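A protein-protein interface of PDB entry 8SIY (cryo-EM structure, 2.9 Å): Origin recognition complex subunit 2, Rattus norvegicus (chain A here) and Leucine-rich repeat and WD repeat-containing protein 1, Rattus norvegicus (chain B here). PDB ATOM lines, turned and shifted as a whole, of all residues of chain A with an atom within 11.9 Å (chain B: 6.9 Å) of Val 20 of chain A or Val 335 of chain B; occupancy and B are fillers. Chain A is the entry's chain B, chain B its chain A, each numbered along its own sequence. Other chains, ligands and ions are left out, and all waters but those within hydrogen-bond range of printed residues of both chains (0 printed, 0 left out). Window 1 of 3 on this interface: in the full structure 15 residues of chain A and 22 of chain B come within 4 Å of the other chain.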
ATOM      1  N   SER A  16      22.434  -8.678  25.407  1.00  0.00           N
ATOM      2  CA  SER A  16      21.106  -8.231  25.020  1.00  0.00           C
ATOM      3  C   SER A  16      20.349  -9.373  24.345  1.00  0.00           C
ATOM      4  O   SER A  16      20.908 -10.426  24.029  1.00  0.00           O
ATOM      5  CB  SER A  16      21.198  -7.028  24.085  1.00  0.00           C
ATOM      6  OG  SER A  16      21.935  -7.349  22.918  1.00  0.00           O
ATOM      7  N   VAL A  17      19.052  -9.159  24.124  1.00  0.00           N
ATOM      8  CA  VAL A  17      18.242 -10.180  23.476  1.00  0.00           C
ATOM      9  C   VAL A  17      18.569 -10.203  21.991  1.00  0.00           C
ATOM     10  O   VAL A  17      18.549  -9.166  21.316  1.00  0.00           O
ATOM     11  CB  VAL A  17      16.746  -9.930  23.719  1.00  0.00           C
ATOM     12  CG1 VAL A  17      16.480  -9.650  25.194  1.00  0.00           C
ATOM     13  CG2 VAL A  17      16.239  -8.796  22.845  1.00  0.00           C
ATOM     14  N   GLN A  18      18.884 -11.388  21.480  1.00  0.00           N
ATOM     15  CA  GLN A  18      19.258 -11.575  20.084  1.00  0.00           C
ATOM     16  C   GLN A  18      18.068 -12.146  19.324  1.00  0.00           C
ATOM     17  O   GLN A  18      17.596 -13.243  19.638  1.00  0.00           O
ATOM     18  CB  GLN A  18      20.467 -12.504  19.973  1.00  0.00           C
ATOM     19  CG  GLN A  18      20.895 -12.801  18.549  1.00  0.00           C
ATOM     20  CD  GLN A  18      21.332 -11.558  17.806  1.00  0.00           C
ATOM     21  OE1 GLN A  18      22.170 -10.795  18.287  1.00  0.00           O
ATOM     22  NE2 GLN A  18      20.762 -11.343  16.627  1.00  0.00           N
ATOM     23  N   PHE A  19      17.586 -11.403  18.330  1.00  0.00           N
ATOM     24  CA  PHE A  19      16.502 -11.881  17.486  1.00  0.00           C
ATOM     25  C   PHE A  19      17.048 -12.792  16.398  1.00  0.00           C
ATOM     26  O   PHE A  19      18.084 -12.501  15.793  1.00  0.00           O
ATOM     27  CB  PHE A  19      15.749 -10.720  16.850  1.00  0.00           C
ATOM     28  CG  PHE A  19      14.814 -11.148  15.758  1.00  0.00           C
ATOM     29  CD1 PHE A  19      13.585 -11.705  16.061  1.00  0.00           C
ATOM     30  CD2 PHE A  19      15.168 -11.010  14.428  1.00  0.00           C
ATOM     31  CE1 PHE A  19      12.723 -12.106  15.062  1.00  0.00           C
ATOM     32  CE2 PHE A  19      14.310 -11.412  13.423  1.00  0.00           C
ATOM     33  CZ  PHE A  19      13.087 -11.960  13.741  1.00  0.00           C
ATOM     34  N   VAL A  20      16.348 -13.891  16.149  1.00  0.00           N
ATOM     35  CA  VAL A  20      16.732 -14.862  15.132  1.00  0.00           C
ATOM     36  C   VAL A  20      15.506 -15.089  14.258  1.00  0.00           C
ATOM     37  O   VAL A  20      14.585 -15.822  14.641  1.00  0.00           O
ATOM     38  CB  VAL A  20      17.237 -16.171  15.746  1.00  0.00           C
ATOM     39  CG1 VAL A  20      17.908 -17.026  14.693  1.00  0.00           C
ATOM     40  CG2 VAL A  20      18.196 -15.879  16.885  1.00  0.00           C
ATOM     41  N   GLY A  21      15.483 -14.460  13.083  1.00  0.00           N
ATOM     42  CA  GLY A  21      14.372 -14.623  12.174  1.00  0.00           C
ATOM     43  C   GLY A  21      14.469 -15.892  11.353  1.00  0.00           C
ATOM     44  O   GLY A  21      15.464 -16.614  11.382  1.00  0.00           O
ATOM     45  N   ASP A  22      13.398 -16.152  10.600  1.00  0.00           N
ATOM     46  CA  ASP A  22      13.327 -17.373   9.804  1.00  0.00           C
ATOM     47  C   ASP A  22      14.506 -17.489   8.852  1.00  0.00           C
ATOM     48  O   ASP A  22      14.964 -18.600   8.562  1.00  0.00           O
ATOM     49  CB  ASP A  22      12.019 -17.403   9.021  1.00  0.00           C
ATOM     50  CG  ASP A  22      10.805 -17.402   9.921  1.00  0.00           C
ATOM     51  OD1 ASP A  22      10.977 -17.394  11.160  1.00  0.00           O
ATOM     52  OD2 ASP A  22       9.674 -17.413   9.387  1.00  0.00           O
ATOM     53  N   ASP A  23      15.012 -16.360   8.361  1.00  0.00           N
ATOM     54  CA  ASP A  23      16.170 -16.349   7.480  1.00  0.00           C
ATOM     55  C   ASP A  23      17.481 -16.570   8.222  1.00  0.00           C
ATOM     56  O   ASP A  23      18.503 -16.821   7.576  1.00  0.00           O
ATOM     57  CB  ASP A  23      16.228 -15.018   6.728  1.00  0.00           C
ATOM     58  CG  ASP A  23      14.995 -14.779   5.876  1.00  0.00           C
ATOM     59  OD1 ASP A  23      14.531 -15.735   5.219  1.00  0.00           O
ATOM     60  OD2 ASP A  23      14.485 -13.639   5.870  1.00  0.00           O
ATOM     61  N   ASP A  24      17.475 -16.489   9.552  1.00  0.00           N
ATOM     62  CA  ASP A  24      18.684 -16.689  10.337  1.00  0.00           C
ATOM     63  C   ASP A  24      18.918 -18.144  10.702  1.00  0.00           C
ATOM     64  O   ASP A  24      20.041 -18.501  11.078  1.00  0.00           O
ATOM     65  CB  ASP A  24      18.619 -15.870  11.629  1.00  0.00           C
ATOM     66  CG  ASP A  24      18.617 -14.380  11.378  1.00  0.00           C
ATOM     67  OD1 ASP A  24      19.105 -13.954  10.311  1.00  0.00           O
ATOM     68  OD2 ASP A  24      18.133 -13.634  12.253  1.00  0.00           O
ATOM     69  N   VAL A  25      17.892 -18.987  10.611  1.00  0.00           N
ATOM     70  CA  VAL A  25      18.065 -20.391  10.941  1.00  0.00           C
ATOM     71  C   VAL A  25      19.069 -21.009   9.984  1.00  0.00           C
ATOM     72  O   VAL A  25      19.074 -20.714   8.781  1.00  0.00           O
ATOM     73  CB  VAL A  25      16.719 -21.128  10.874  1.00  0.00           C
ATOM     74  CG1 VAL A  25      16.317 -21.331   9.446  1.00  0.00           C
ATOM     75  CG2 VAL A  25      16.800 -22.462  11.579  1.00  0.00           C
ATOM     76  N   LEU A  26      19.934 -21.870  10.516  1.00  0.00           N
ATOM     77  CA  LEU A  26      20.887 -22.564   9.663  1.00  0.00           C
ATOM     78  C   LEU A  26      20.189 -23.565   8.752  1.00  0.00           C
ATOM     79  O   LEU A  26      20.630 -23.781   7.618  1.00  0.00           O
ATOM     80  CB  LEU A  26      21.943 -23.266  10.517  1.00  0.00           C
ATOM     81  CG  LEU A  26      22.741 -22.406  11.502  1.00  0.00           C
ATOM     82  CD1 LEU A  26      23.895 -23.208  12.073  1.00  0.00           C
ATOM     83  CD2 LEU A  26      23.246 -21.136  10.850  1.00  0.00           C
ATOM     84  N   SER A  27      19.110 -24.187   9.226  1.00  0.00           N
ATOM     85  CA  SER A  27      18.366 -25.157   8.438  1.00  0.00           C
ATOM     86  C   SER A  27      16.915 -25.167   8.896  1.00  0.00           C
ATOM     87  O   SER A  27      16.634 -25.014  10.086  1.00  0.00           O
ATOM     88  CB  SER A  27      18.960 -26.564   8.571  1.00  0.00           C
ATOM     89  OG  SER A  27      18.257 -27.488   7.761  1.00  0.00           O
ATOM     90  N   HIS A  28      16.004 -25.357   7.948  1.00  0.00           N
ATOM     91  CA  HIS A  28      14.589 -25.522   8.243  1.00  0.00           C
ATOM     92  C   HIS A  28      14.222 -26.999   8.174  1.00  0.00           C
ATOM     93  O   HIS A  28      14.634 -27.706   7.250  1.00  0.00           O
ATOM     94  CB  HIS A  28      13.719 -24.738   7.256  1.00  0.00           C
ATOM     95  CG  HIS A  28      13.866 -23.249   7.346  1.00  0.00           C
ATOM     96  ND1 HIS A  28      12.968 -22.454   8.025  1.00  0.00           N
ATOM     97  CD2 HIS A  28      14.788 -22.410   6.818  1.00  0.00           C
ATOM     98  CE1 HIS A  28      13.335 -21.189   7.920  1.00  0.00           C
ATOM     99  NE2 HIS A  28      14.437 -21.134   7.193  1.00  0.00           N
ATOM    100  N   ILE A  29      13.457 -27.460   9.155  1.00  0.00           N
ATOM    101  CA  ILE A  29      12.859 -28.787   9.099  1.00  0.00           C
ATOM    102  C   ILE A  29      11.644 -28.735   8.183  1.00  0.00           C
ATOM    103  O   ILE A  29      10.831 -27.806   8.262  1.00  0.00           O
ATOM    104  CB  ILE A  29      12.462 -29.259  10.509  1.00  0.00           C
ATOM    105  CG1 ILE A  29      13.659 -29.195  11.463  1.00  0.00           C
ATOM    106  CG2 ILE A  29      11.871 -30.663  10.463  1.00  0.00           C
ATOM    107  CD1 ILE A  29      14.845 -30.025  11.029  1.00  0.00           C
ATOM    108  N   PHE B 279      20.690 -14.731  25.117  1.00  0.00           N
ATOM    109  CA  PHE B 279      19.264 -14.430  25.208  1.00  0.00           C
ATOM    110  C   PHE B 279      18.738 -14.391  23.777  1.00  0.00           C
ATOM    111  O   PHE B 279      18.898 -13.385  23.081  1.00  0.00           O
ATOM    112  CB  PHE B 279      19.009 -13.118  25.942  1.00  0.00           C
ATOM    113  CG  PHE B 279      19.424 -13.144  27.385  1.00  0.00           C
ATOM    114  CD1 PHE B 279      18.555 -13.603  28.361  1.00  0.00           C
ATOM    115  CD2 PHE B 279      20.681 -12.712  27.767  1.00  0.00           C
ATOM    116  CE1 PHE B 279      18.933 -13.629  29.690  1.00  0.00           C
ATOM    117  CE2 PHE B 279      21.065 -12.735  29.096  1.00  0.00           C
ATOM    118  CZ  PHE B 279      20.189 -13.195  30.058  1.00  0.00           C
ATOM    119  N   LEU B 280      18.118 -15.486  23.343  1.00  0.00           N
ATOM    120  CA  LEU B 280      17.728 -15.677  21.952  1.00  0.00           C
ATOM    121  C   LEU B 280      16.223 -15.515  21.797  1.00  0.00           C
ATOM    122  O   LEU B 280      15.452 -16.015  22.622  1.00  0.00           O
ATOM    123  CB  LEU B 280      18.154 -17.061  21.463  1.00  0.00           C
ATOM    124  CG  LEU B 280      19.629 -17.409  21.661  1.00  0.00           C
ATOM    125  CD1 LEU B 280      19.914 -18.809  21.141  1.00  0.00           C
ATOM    126  CD2 LEU B 280      20.518 -16.387  20.977  1.00  0.00           C
ATOM    127  N   GLN B 281      15.811 -14.817  20.741  1.00  0.00           N
ATOM    128  CA  GLN B 281      14.403 -14.640  20.394  1.00  0.00           C
ATOM    129  C   GLN B 281      14.186 -15.285  19.026  1.00  0.00           C
ATOM    130  O   GLN B 281      14.416 -14.661  17.988  1.00  0.00           O
ATOM    131  CB  GLN B 281      14.030 -13.162  20.395  1.00  0.00           C
ATOM    132  CG  GLN B 281      12.570 -12.879  20.095  1.00  0.00           C
ATOM    133  CD  GLN B 281      12.303 -11.406  19.860  1.00  0.00           C
ATOM    134  OE1 GLN B 281      13.230 -10.605  19.750  1.00  0.00           O
ATOM    135  NE2 GLN B 281      11.030 -11.040  19.781  1.00  0.00           N
ATOM    136  N   CYS B 282      13.731 -16.542  19.029  1.00  0.00           N
ATOM    137  CA  CYS B 282      13.649 -17.334  17.808  1.00  0.00           C
ATOM    138  C   CYS B 282      12.289 -17.986  17.586  1.00  0.00           C
ATOM    139  O   CYS B 282      12.131 -18.726  16.609  1.00  0.00           O
ATOM    140  CB  CYS B 282      14.737 -18.415  17.817  1.00  0.00           C
ATOM    141  SG  CYS B 282      14.820 -19.356  19.358  1.00  0.00           S
ATOM    142  N   HIS B 283      11.305 -17.735  18.449  1.00  0.00           N
ATOM    143  CA  HIS B 283       9.959 -18.279  18.299  1.00  0.00           C
ATOM    144  C   HIS B 283       8.944 -17.164  18.072  1.00  0.00           C
ATOM    145  O   HIS B 283       7.819 -17.211  18.571  1.00  0.00           O
ATOM    146  CB  HIS B 283       9.558 -19.109  19.515  1.00  0.00           C
ATOM    147  CG  HIS B 283      10.530 -20.192  19.864  1.00  0.00           C
ATOM    148  ND1 HIS B 283      11.700 -19.950  20.551  1.00  0.00           N
ATOM    149  CD2 HIS B 283      10.498 -21.526  19.635  1.00  0.00           C
ATOM    150  CE1 HIS B 283      12.350 -21.086  20.723  1.00  0.00           C
ATOM    151  NE2 HIS B 283      11.642 -22.058  20.177  1.00  0.00           N
ATOM    152  N   SER B 284       9.338 -16.139  17.323  1.00  0.00           N
ATOM    153  CA  SER B 284       8.432 -15.036  17.035  1.00  0.00           C
ATOM    154  C   SER B 284       7.257 -15.507  16.190  1.00  0.00           C
ATOM    155  O   SER B 284       7.396 -16.351  15.301  1.00  0.00           O
ATOM    156  CB  SER B 284       9.173 -13.913  16.310  1.00  0.00           C
ATOM    157  OG  SER B 284       9.868 -13.088  17.226  1.00  0.00           O
ATOM    158  N   ASN B 287       6.979 -14.109  12.416  1.00  0.00           N
ATOM    159  CA  ASN B 287       8.387 -13.751  12.261  1.00  0.00           C
ATOM    160  C   ASN B 287       8.605 -12.268  12.562  1.00  0.00           C
ATOM    161  O   ASN B 287       9.385 -11.581  11.901  1.00  0.00           O
ATOM    162  CB  ASN B 287       8.892 -14.105  10.863  1.00  0.00           C
ATOM    163  CG  ASN B 287      10.385 -13.890  10.713  1.00  0.00           C
ATOM    164  OD1 ASN B 287      11.140 -14.022  11.674  1.00  0.00           O
ATOM    165  ND2 ASN B 287      10.818 -13.555   9.505  1.00  0.00           N
ATOM    166  N   CYS B 326      12.350 -25.262  18.098  1.00  0.00           N
ATOM    167  CA  CYS B 326      13.688 -24.794  17.774  1.00  0.00           C
ATOM    168  C   CYS B 326      14.736 -25.698  18.409  1.00  0.00           C
ATOM    169  O   CYS B 326      14.571 -26.175  19.536  1.00  0.00           O
ATOM    170  CB  CYS B 326      13.896 -23.351  18.245  1.00  0.00           C
ATOM    171  SG  CYS B 326      12.906 -22.133  17.349  1.00  0.00           S
ATOM    172  N   VAL B 327      15.821 -25.922  17.671  1.00  0.00           N
ATOM    173  CA  VAL B 327      16.969 -26.683  18.146  1.00  0.00           C
ATOM    174  C   VAL B 327      18.154 -25.732  18.194  1.00  0.00           C
ATOM    175  O   VAL B 327      18.594 -25.228  17.153  1.00  0.00           O
ATOM    176  CB  VAL B 327      17.263 -27.895  17.250  1.00  0.00           C
ATOM    177  CG1 VAL B 327      18.428 -28.699  17.807  1.00  0.00           C
ATOM    178  CG2 VAL B 327      16.018 -28.763  17.124  1.00  0.00           C
ATOM    179  N   ILE B 328      18.676 -25.502  19.397  1.00  0.00           N
ATOM    180  CA  ILE B 328      19.609 -24.418  19.674  1.00  0.00           C
ATOM    181  C   ILE B 328      20.896 -24.997  20.237  1.00  0.00           C
ATOM    182  O   ILE B 328      20.867 -25.923  21.055  1.00  0.00           O
ATOM    183  CB  ILE B 328      19.006 -23.400  20.665  1.00  0.00           C
ATOM    184  CG1 ILE B 328      17.662 -22.882  20.149  1.00  0.00           C
ATOM    185  CG2 ILE B 328      19.979 -22.250  20.904  1.00  0.00           C
ATOM    186  CD1 ILE B 328      16.936 -21.979  21.126  1.00  0.00           C
ATOM    187  N   ASP B 329      22.023 -24.452  19.795  1.00  0.00           N
ATOM    188  CA  ASP B 329      23.322 -24.762  20.381  1.00  0.00           C
ATOM    189  C   ASP B 329      23.581 -23.767  21.509  1.00  0.00           C
ATOM    190  O   ASP B 329      23.815 -22.580  21.255  1.00  0.00           O
ATOM    191  CB  ASP B 329      24.416 -24.703  19.320  1.00  0.00           C
ATOM    192  CG  ASP B 329      25.809 -24.747  19.915  1.00  0.00           C
ATOM    193  OD1 ASP B 329      26.289 -25.856  20.234  1.00  0.00           O
ATOM    194  OD2 ASP B 329      26.420 -23.670  20.067  1.00  0.00           O
ATOM    195  N   THR B 332      27.182 -21.705  21.107  1.00  0.00           N
ATOM    196  CA  THR B 332      27.314 -20.680  20.082  1.00  0.00           C
ATOM    197  C   THR B 332      26.086 -19.793  19.943  1.00  0.00           C
ATOM    198  O   THR B 332      26.191 -18.700  19.377  1.00  0.00           O
ATOM    199  CB  THR B 332      27.598 -21.334  18.730  1.00  0.00           C
ATOM    200  OG1 THR B 332      26.526 -22.226  18.401  1.00  0.00           O
ATOM    201  CG2 THR B 332      28.907 -22.108  18.780  1.00  0.00           C
ATOM    202  N   GLY B 333      24.930 -20.234  20.426  1.00  0.00           N
ATOM    203  CA  GLY B 333      23.714 -19.467  20.299  1.00  0.00           C
ATOM    204  C   GLY B 333      23.045 -19.546  18.945  1.00  0.00           C
ATOM    205  O   GLY B 333      21.992 -18.925  18.758  1.00  0.00           O
ATOM    206  N   LEU B 334      23.611 -20.288  17.998  1.00  0.00           N
ATOM    207  CA  LEU B 334      22.966 -20.461  16.704  1.00  0.00           C
ATOM    208  C   LEU B 334      21.775 -21.399  16.833  1.00  0.00           C
ATOM    209  O   LEU B 334      21.836 -22.411  17.535  1.00  0.00           O
ATOM    210  CB  LEU B 334      23.964 -21.022  15.685  1.00  0.00           C
ATOM    211  CG  LEU B 334      25.171 -20.136  15.364  1.00  0.00           C
ATOM    212  CD1 LEU B 334      26.186 -20.860  14.484  1.00  0.00           C
ATOM    213  CD2 LEU B 334      24.700 -18.859  14.698  1.00  0.00           C
ATOM    214  N   VAL B 335      20.686 -21.069  16.147  1.00  0.00           N
ATOM    215  CA  VAL B 335      19.522 -21.945  16.089  1.00  0.00           C
ATOM    216  C   VAL B 335      19.737 -22.908  14.928  1.00  0.00           C
ATOM    217  O   VAL B 335      19.740 -22.510  13.762  1.00  0.00           O
ATOM    218  CB  VAL B 335      18.212 -21.158  15.947  1.00  0.00           C
ATOM    219  CG1 VAL B 335      17.982 -20.280  17.173  1.00  0.00           C
ATOM    220  CG2 VAL B 335      18.204 -20.313  14.683  1.00  0.00           C
ATOM    221  N   LEU B 336      19.934 -24.185  15.255  1.00  0.00           N
ATOM    222  CA  LEU B 336      20.306 -25.162  14.240  1.00  0.00           C
ATOM    223  C   LEU B 336      19.120 -25.538  13.363  1.00  0.00           C
ATOM    224  O   LEU B 336      19.275 -25.723  12.150  1.00  0.00           O
ATOM    225  CB  LEU B 336      20.887 -26.405  14.909  1.00  0.00           C
ATOM    226  CG  LEU B 336      22.098 -26.164  15.816  1.00  0.00           C
ATOM    227  CD1 LEU B 336      22.501 -27.446  16.524  1.00  0.00           C
ATOM    228  CD2 LEU B 336      23.265 -25.602  15.023  1.00  0.00           C
ATOM    229  N   HIS B 337      17.936 -25.692  13.955  1.00  0.00           N
ATOM    230  CA  HIS B 337      16.775 -26.162  13.218  1.00  0.00           C
ATOM    231  C   HIS B 337      15.508 -25.537  13.777  1.00  0.00           C
ATOM    232  O   HIS B 337      15.408 -25.235  14.970  1.00  0.00           O
ATOM    233  CB  HIS B 337      16.673 -27.689  13.256  1.00  0.00           C
ATOM    234  CG  HIS B 337      17.871 -28.374  12.682  1.00  0.00           C
ATOM    235  ND1 HIS B 337      17.945 -28.760  11.362  1.00  0.00           N
ATOM    236  CD2 HIS B 337      19.056 -28.714  13.241  1.00  0.00           C
ATOM    237  CE1 HIS B 337      19.118 -29.321  11.135  1.00  0.00           C
ATOM    238  NE2 HIS B 337      19.812 -29.305  12.259  1.00  0.00           N
ATOM    239  N   LYS B 338      14.545 -25.340  12.885  1.00  0.00           N
ATOM    240  CA  LYS B 338      13.257 -24.774  13.242  1.00  0.00           C
ATOM    241  C   LYS B 338      12.181 -25.438  12.400  1.00  0.00           C
ATOM    242  O   LYS B 338      12.326 -25.567  11.181  1.00  0.00           O
ATOM    243  CB  LYS B 338      13.246 -23.255  13.048  1.00  0.00           C
ATOM    244  CG  LYS B 338      11.990 -22.574  13.569  1.00  0.00           C
ATOM    245  CD  LYS B 338      12.033 -21.067  13.354  1.00  0.00           C
ATOM    246  CE  LYS B 338      10.818 -20.382  13.961  1.00  0.00           C
ATOM    247  NZ  LYS B 338      10.822 -18.916  13.696  1.00  0.00           N
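The backbone carbonyl oxygen (O) of Gln 281 of chain B lies within hydrogen-bond range of the backbone NH (N) of Val 20 of chain A (2.8 Å).
The backbone NH (N) of Gln 281 of chain B lies within hydrogen-bond range of the backbone carbonyl oxygen (O) of Gln 18 of chain A (2.6 Å).
O of Lys 338 of chain B is in hydrogen-bond range of N of Ile 29 of chain A, at 3.0 Å.
N of Gln 18 of chain A is in hydrogen-bond range of O of Phe 279 of chain B (2.6 Å).
The side-chain amino group of Lys 338 of chain B is in salt-bridge range of the side-chain carboxylate of Asp 22 of chain A, at 3.0 Å.
The backbone NH (N) of Leu 26 of chain A sits at hydrogen-bond distance from the backbone carbonyl oxygen (O) of Val 335 of chain B, 3.3 Å away.
The backbone NH (N) of Asp 22 of chain A is in hydrogen-bond range of the side-chain amide oxygen (OD1) of Asn 287 of chain B (3.3 Å).
The backbone NH (N) of Ser 27 of chain A is in hydrogen-bond range of the backbone carbonyl oxygen (O) of Leu 336 of chain B, at 3.3 Å.
O of Asp 22 of chain A sits at hydrogen-bond distance from NE2 of His 28 of chain A, 2.9 Å away.
SG of Cys 282 of chain B sits close to ND1 of His 283 of chain B.
NE2 of Gln 281 of chain B sits at hydrogen-bond distance from OG of Ser 284 of chain B.
The backbone NH (N) of Leu 336 of chain B sits at hydrogen-bond distance from the backbone carbonyl oxygen (O) of Val 327 of chain B (2.5 Å).
The backbone NH (N) of Val 327 of chain B is in hydrogen-bond range of the backbone carbonyl oxygen (O) of His 337 of chain B (2.8 Å).
The backbone NH (N) of Gly 21 of chain A is in hydrogen-bond range of the side-chain carboxylate (OD2) of Asp 24 of chain A (2.9 Å).
Among the printed residues, pairs that only touch across the chains: Ser 16 of chain A with Phe 279 of chain B (3.7 Å), Val 17 of chain A with Phe 279 of chain B (3.3 Å), Gln 18 of chain A with Leu 280 of chain B (3.4 Å), Phe 19 of chain A with Gln 281 of chain B (3.5 Å), Phe 19 of chain A with Ser 284 of chain B (3.7 Å), Phe 19 of chain A with Asn 287 of chain B (3.5 Å), Val 20 of chain A with Cys 282 of chain B (3.6 Å), Val 20 of chain A with Val 335 of chain B (3.3 Å), Gly 21 of chain A with Asn 287 of chain B (3.3 Å), Val 25 of chain A with Val 335 of chain B (3.7 Å), Val 25 of chain A with His 337 of chain B (3.99 Å), Val 25 of chain A with Lys 338 of chain B (3.9 Å), Leu 26 of chain A with Leu 336 of chain B (3.9 Å), Ser 27 of chain A with His 337 of chain B (3.3 Å), Ser 27 of chain A with Lys 338 of chain B (3.5 Å), His 28 of chain A with Lys 338 of chain B (3.7 Å) and Ile 29 of chain A with His 337 of chain B (3.4 Å).
Val 20 of chain A touches just these residues of chain B: Gln 281, Cys 282 and Val 335.
Of the printed residues of chain B, Asp 22 of chain A touches Asn 287 and Lys 338.
Asp 24 of chain A touches none of the printed residues of chain B.
Of the printed residues of chain A, Leu 280 of chain B touches Gln 18 (3.4 Å).
Of chain A, only Gln 18, Phe 19 and Val 20 come within 4 Å of Gln 281 of chain B.
No residue of chain A comes within 4 Å of Val 327 of chain B.
Gly 333 of chain B touches none of the printed residues of chain A.
No residue of chain A comes within 4 Å of Leu 334 of chain B.
Val 335 of chain B touches just these residues of chain A: Val 20 (3.3 Å), Val 25 (3.7 Å) and Leu 26 (3.3 Å).
Of chain A, only Leu 26 (3.9 Å) and Ser 27 (3.3 Å) come within 4 Å of Leu 336 of chain B.
Of the printed residues of chain A, Lys 338 of chain B touches Asp 22 (3.0 Å), Val 25 (3.9 Å), Ser 27 (3.5 Å), His 28 (3.7 Å) and Ile 29 (3.0 Å).
The nearest residue of chain B that does not touch Val 20 of chain A is Leu 280 of chain B (4.7 Å).
Printed residues of chain B that touch a printed residue of chain A: Phe 279, Leu 280, Gln 281, Cys 282, Ser 284, Asn 287, Val 335, Leu 336, His 337 and Lys 338.
Hydrophobic or aromatic side chains of chain B that line the printed part of chain A: Phe 279, Val 335, Leu 336 and His 337.
Printed residues of chain A that touch a printed residue of chain B: Ser 16, Val 17, Gln 18, Phe 19, Val 20, Gly 21, Asp 22, Val 25, Leu 26, Ser 27, His 28 and Ile 29.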
